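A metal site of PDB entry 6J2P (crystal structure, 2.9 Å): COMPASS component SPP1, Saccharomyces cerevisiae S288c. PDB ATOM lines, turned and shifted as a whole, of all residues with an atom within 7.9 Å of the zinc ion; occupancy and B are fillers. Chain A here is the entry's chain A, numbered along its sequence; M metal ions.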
ATOM      1  N   GLY A  41     -25.500  24.524  20.093  1.00  0.00           N
ATOM      2  CA  GLY A  41     -26.162  24.866  18.855  1.00  0.00           C
ATOM      3  C   GLY A  41     -25.445  26.008  18.180  1.00  0.00           C
ATOM      4  O   GLY A  41     -25.174  27.044  18.804  1.00  0.00           O
ATOM      5  N   CYS A  42     -25.114  25.821  16.908  1.00  0.00           N
ATOM      6  CA  CYS A  42     -24.469  26.882  16.140  1.00  0.00           C
ATOM      7  C   CYS A  42     -25.448  28.025  15.901  1.00  0.00           C
ATOM      8  O   CYS A  42     -26.664  27.835  15.863  1.00  0.00           O
ATOM      9  CB  CYS A  42     -23.940  26.349  14.814  1.00  0.00           C
ATOM     10  SG  CYS A  42     -22.915  27.527  13.897  1.00  0.00           S
ATOM     11  N   ASP A  43     -24.902  29.228  15.739  1.00  0.00           N
ATOM     12  CA  ASP A  43     -25.729  30.406  15.494  1.00  0.00           C
ATOM     13  C   ASP A  43     -25.773  30.804  14.027  1.00  0.00           C
ATOM     14  O   ASP A  43     -26.687  31.536  13.629  1.00  0.00           O
ATOM     15  CB  ASP A  43     -25.224  31.585  16.331  1.00  0.00           C
ATOM     16  CG  ASP A  43     -25.601  31.467  17.796  1.00  0.00           C
ATOM     17  OD1 ASP A  43     -26.753  31.066  18.074  1.00  0.00           O
ATOM     18  OD2 ASP A  43     -24.762  31.763  18.661  1.00  0.00           O
ATOM     19  N   GLY A  44     -24.826  30.331  13.211  1.00  0.00           N
ATOM     20  CA  GLY A  44     -24.912  30.535  11.772  1.00  0.00           C
ATOM     21  C   GLY A  44     -25.980  29.653  11.175  1.00  0.00           C
ATOM     22  O   GLY A  44     -27.059  30.124  10.807  1.00  0.00           O
ATOM     23  N   CYS A  45     -25.688  28.353  11.068  1.00  0.00           N
ATOM     24  CA  CYS A  45     -26.714  27.369  10.774  1.00  0.00           C
ATOM     25  C   CYS A  45     -27.410  26.980  12.068  1.00  0.00           C
ATOM     26  O   CYS A  45     -27.064  27.448  13.165  1.00  0.00           O
ATOM     27  CB  CYS A  45     -26.098  26.156  10.084  1.00  0.00           C
ATOM     28  SG  CYS A  45     -24.939  25.214  11.118  1.00  0.00           S
ATOM     29  N   ASP A  46     -28.417  26.123  11.969  1.00  0.00           N
ATOM     30  CA  ASP A  46     -29.151  25.657  13.140  1.00  0.00           C
ATOM     31  C   ASP A  46     -28.803  24.207  13.487  1.00  0.00           C
ATOM     32  O   ASP A  46     -29.679  23.403  13.801  1.00  0.00           O
ATOM     33  CB  ASP A  46     -30.653  25.817  12.949  1.00  0.00           C
ATOM     34  CG  ASP A  46     -31.398  25.935  14.260  1.00  0.00           C
ATOM     35  OD1 ASP A  46     -32.007  24.934  14.692  1.00  0.00           O
ATOM     36  OD2 ASP A  46     -31.373  27.023  14.861  1.00  0.00           O
ATOM     37  N   ASP A  47     -27.518  23.879  13.420  1.00  0.00           N
ATOM     38  CA  ASP A  47     -27.052  22.533  13.743  1.00  0.00           C
ATOM     39  C   ASP A  47     -26.607  22.467  15.203  1.00  0.00           C
ATOM     40  O   ASP A  47     -26.544  23.470  15.921  1.00  0.00           O
ATOM     41  CB  ASP A  47     -25.926  22.120  12.807  1.00  0.00           C
ATOM     42  CG  ASP A  47     -25.891  20.622  12.555  1.00  0.00           C
ATOM     43  OD1 ASP A  47     -25.119  20.182  11.668  1.00  0.00           O
ATOM     44  OD2 ASP A  47     -26.634  19.885  13.240  1.00  0.00           O
ATOM     45  N   TRP A  48     -26.281  21.248  15.639  1.00  0.00           N
ATOM     46  CA  TRP A  48     -25.823  20.994  17.005  1.00  0.00           C
ATOM     47  C   TRP A  48     -24.573  20.140  16.951  1.00  0.00           C
ATOM     48  O   TRP A  48     -24.469  19.233  16.130  1.00  0.00           O
ATOM     49  CB  TRP A  48     -26.914  20.311  17.831  1.00  0.00           C
ATOM     50  CG  TRP A  48     -28.096  21.205  18.068  1.00  0.00           C
ATOM     51  CD1 TRP A  48     -29.119  21.445  17.197  1.00  0.00           C
ATOM     52  CD2 TRP A  48     -28.371  21.975  19.243  1.00  0.00           C
ATOM     53  NE1 TRP A  48     -30.011  22.324  17.769  1.00  0.00           N
ATOM     54  CE2 TRP A  48     -29.579  22.663  19.023  1.00  0.00           C
ATOM     55  CE3 TRP A  48     -27.702  22.148  20.457  1.00  0.00           C
ATOM     56  CZ2 TRP A  48     -30.135  23.514  19.975  1.00  0.00           C
ATOM     57  CZ3 TRP A  48     -28.265  22.997  21.404  1.00  0.00           C
ATOM     58  CH2 TRP A  48     -29.466  23.663  21.149  1.00  0.00           C
ATOM     59  N   PHE A  49     -23.621  20.443  17.836  1.00  0.00           N
ATOM     60  CA  PHE A  49     -22.293  19.854  17.780  1.00  0.00           C
ATOM     61  C   PHE A  49     -21.862  19.374  19.151  1.00  0.00           C
ATOM     62  O   PHE A  49     -22.031  20.091  20.145  1.00  0.00           O
ATOM     63  CB  PHE A  49     -21.268  20.857  17.216  1.00  0.00           C
ATOM     64  CG  PHE A  49     -21.626  21.366  15.841  1.00  0.00           C
ATOM     65  CD1 PHE A  49     -21.074  20.797  14.717  1.00  0.00           C
ATOM     66  CD2 PHE A  49     -22.518  22.422  15.692  1.00  0.00           C
ATOM     67  CE1 PHE A  49     -21.398  21.257  13.451  1.00  0.00           C
ATOM     68  CE2 PHE A  49     -22.851  22.885  14.436  1.00  0.00           C
ATOM     69  CZ  PHE A  49     -22.295  22.308  13.310  1.00  0.00           C
ATOM     70  N   PHE A  67     -21.711  30.513  19.860  1.00  0.00           N
ATOM     71  CA  PHE A  67     -20.859  29.516  19.218  1.00  0.00           C
ATOM     72  C   PHE A  67     -21.082  29.527  17.712  1.00  0.00           C
ATOM     73  O   PHE A  67     -22.218  29.684  17.236  1.00  0.00           O
ATOM     74  CB  PHE A  67     -21.126  28.120  19.783  1.00  0.00           C
ATOM     75  CG  PHE A  67     -20.431  27.026  19.028  1.00  0.00           C
ATOM     76  CD1 PHE A  67     -19.073  26.810  19.192  1.00  0.00           C
ATOM     77  CD2 PHE A  67     -21.136  26.207  18.160  1.00  0.00           C
ATOM     78  CE1 PHE A  67     -18.426  25.801  18.501  1.00  0.00           C
ATOM     79  CE2 PHE A  67     -20.502  25.204  17.465  1.00  0.00           C
ATOM     80  CZ  PHE A  67     -19.141  24.999  17.637  1.00  0.00           C
ATOM     81  N   TYR A  68     -20.000  29.352  16.960  1.00  0.00           N
ATOM     82  CA  TYR A  68     -20.047  29.241  15.509  1.00  0.00           C
ATOM     83  C   TYR A  68     -19.195  28.050  15.092  1.00  0.00           C
ATOM     84  O   TYR A  68     -18.000  28.009  15.397  1.00  0.00           O
ATOM     85  CB  TYR A  68     -19.560  30.528  14.839  1.00  0.00           C
ATOM     86  CG  TYR A  68     -20.569  31.655  14.913  1.00  0.00           C
ATOM     87  CD1 TYR A  68     -21.701  31.642  14.113  1.00  0.00           C
ATOM     88  CD2 TYR A  68     -20.393  32.716  15.799  1.00  0.00           C
ATOM     89  CE1 TYR A  68     -22.633  32.673  14.175  1.00  0.00           C
ATOM     90  CE2 TYR A  68     -21.317  33.736  15.872  1.00  0.00           C
ATOM     91  CZ  TYR A  68     -22.435  33.711  15.059  1.00  0.00           C
ATOM     92  OH  TYR A  68     -23.358  34.725  15.116  1.00  0.00           O
ATOM     93  N   CYS A  69     -19.824  27.085  14.416  1.00  0.00           N
ATOM     94  CA  CYS A  69     -19.142  25.859  14.047  1.00  0.00           C
ATOM     95  C   CYS A  69     -18.010  26.144  13.054  1.00  0.00           C
ATOM     96  O   CYS A  69     -17.979  27.210  12.436  1.00  0.00           O
ATOM     97  CB  CYS A  69     -20.141  24.872  13.453  1.00  0.00           C
ATOM     98  SG  CYS A  69     -20.680  25.224  11.769  1.00  0.00           S
ATOM     99  N   PRO A  70     -17.067  25.216  12.904  1.00  0.00           N
ATOM    100  CA  PRO A  70     -15.955  25.449  11.973  1.00  0.00           C
ATOM    101  C   PRO A  70     -16.401  25.726  10.549  1.00  0.00           C
ATOM    102  O   PRO A  70     -15.739  26.498   9.838  1.00  0.00           O
ATOM    103  CB  PRO A  70     -15.129  24.165  12.061  1.00  0.00           C
ATOM    104  CG  PRO A  70     -16.040  23.153  12.701  1.00  0.00           C
ATOM    105  CD  PRO A  70     -16.899  23.943  13.632  1.00  0.00           C
ATOM    106  N   TYR A  71     -17.509  25.139  10.108  1.00  0.00           N
ATOM    107  CA  TYR A  71     -17.975  25.365   8.746  1.00  0.00           C
ATOM    108  C   TYR A  71     -18.665  26.709   8.578  1.00  0.00           C
ATOM    109  O   TYR A  71     -18.722  27.222   7.451  1.00  0.00           O
ATOM    110  CB  TYR A  71     -18.921  24.225   8.327  1.00  0.00           C
ATOM    111  CG  TYR A  71     -18.230  22.901   8.152  1.00  0.00           C
ATOM    112  CD1 TYR A  71     -17.013  22.809   7.479  1.00  0.00           C
ATOM    113  CD2 TYR A  71     -18.775  21.734   8.666  1.00  0.00           C
ATOM    114  CE1 TYR A  71     -16.375  21.594   7.314  1.00  0.00           C
ATOM    115  CE2 TYR A  71     -18.146  20.510   8.515  1.00  0.00           C
ATOM    116  CZ  TYR A  71     -16.938  20.448   7.842  1.00  0.00           C
ATOM    117  OH  TYR A  71     -16.305  19.242   7.679  1.00  0.00           O
ATOM    118  N   CYS A  72     -19.185  27.297   9.654  1.00  0.00           N
ATOM    119  CA  CYS A  72     -19.767  28.628   9.569  1.00  0.00           C
ATOM    120  C   CYS A  72     -18.696  29.718   9.664  1.00  0.00           C
ATOM    121  O   CYS A  72     -18.831  30.770   9.030  1.00  0.00           O
ATOM    122  CB  CYS A  72     -20.817  28.826  10.656  1.00  0.00           C
ATOM    123  SG  CYS A  72     -22.417  28.052  10.281  1.00  0.00           S
ATOM    124  N   GLN A  73     -17.646  29.483  10.448  1.00  0.00           N
ATOM    125  CA  GLN A  73     -16.532  30.418  10.513  1.00  0.00           C
ATOM    126  C   GLN A  73     -15.739  30.449   9.217  1.00  0.00           C
ATOM    127  O   GLN A  73     -15.016  31.422   8.967  1.00  0.00           O
ATOM    128  CB  GLN A  73     -15.615  30.076  11.692  1.00  0.00           C
ATOM    129  CG  GLN A  73     -16.332  29.992  13.028  1.00  0.00           C
ATOM    130  CD  GLN A  73     -15.388  29.755  14.182  1.00  0.00           C
ATOM    131  OE1 GLN A  73     -14.213  29.443  13.981  1.00  0.00           O
ATOM    132  NE2 GLN A  73     -15.877  29.906  15.403  1.00  0.00           N
ATOM    133  N   THR A  77     -21.372  27.541   5.411  1.00  0.00           N
ATOM    134  CA  THR A  77     -22.766  27.216   5.670  1.00  0.00           C
ATOM    135  C   THR A  77     -23.460  28.208   6.612  1.00  0.00           C
ATOM    136  O   THR A  77     -24.530  27.894   7.137  1.00  0.00           O
ATOM    137  CB  THR A  77     -22.896  25.814   6.260  1.00  0.00           C
ATOM    138  OG1 THR A  77     -24.237  25.604   6.740  1.00  0.00           O
ATOM    139  CG2 THR A  77     -21.929  25.637   7.411  1.00  0.00           C
ATOM    140  N   GLY A  78     -22.876  29.390   6.828  1.00  0.00           N
ATOM    141  CA  GLY A  78     -23.503  30.338   7.718  1.00  0.00           C
ATOM    142  C   GLY A  78     -24.676  31.089   7.111  1.00  0.00           C
ATOM    143  O   GLY A  78     -25.638  30.470   6.645  1.00  0.00           O
ATOM    144  N   LYS A  79     -24.606  32.420   7.125  1.00  0.00           N
ATOM    145  CA  LYS A  79     -25.648  33.230   6.513  1.00  0.00           C
ATOM    146  C   LYS A  79     -25.118  34.560   5.972  1.00  0.00           C
ATOM    147  O   LYS A  79     -25.922  35.434   5.646  1.00  0.00           O
ATOM    148  CB  LYS A  79     -26.780  33.492   7.511  1.00  0.00           C
ATOM    149  N   PRO A  88     -18.320  35.039  11.025  1.00  0.00           N
ATOM    150  CA  PRO A  88     -18.606  34.955  12.460  1.00  0.00           C
ATOM    151  C   PRO A  88     -17.547  34.144  13.187  1.00  0.00           C
ATOM    152  O   PRO A  88     -16.959  33.214  12.640  1.00  0.00           O
ATOM    153  CB  PRO A  88     -19.974  34.261  12.509  1.00  0.00           C
ATOM    154  CG  PRO A  88     -19.995  33.421  11.273  1.00  0.00           C
ATOM    155  CD  PRO A  88     -19.248  34.209  10.228  1.00  0.00           C
HETATM  156 ZN    ZN M   1     -22.957  26.340  11.818  1.00  0.00          ZN
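SG of Cys 72 sits close to N of Gly 78, 3.7 Å away. SG of Cys 42 lies close to N of Gly 44. The backbone NH of Cys 42 is in hydrogen-bond range of the backbone carbonyl oxygen of Asp 47 (2.9 Å). The backbone carbonyl oxygen (O) of Thr 77 lies close to the side-chain sulfur (SG) of Cys 72 (3.8 Å). The side-chain sulfur (SG) of Cys 69 sits close to the backbone NH (N) of Tyr 71 (3.6 Å). SG of Cys 45 sits close to N of Asp 47, at 3.7 Å.
The zinc ion is bound by SG of Cys 72 (2.4 Å), SG of Cys 45 (2.4 Å), SG of Cys 42 (2.4 Å) and SG of Cys 69 (2.5 Å). The zinc ion has four donor atoms within binding distance.
Within 4 Å of the zinc ion: Cys 42, Cys 45, Cys 69 and Cys 72.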
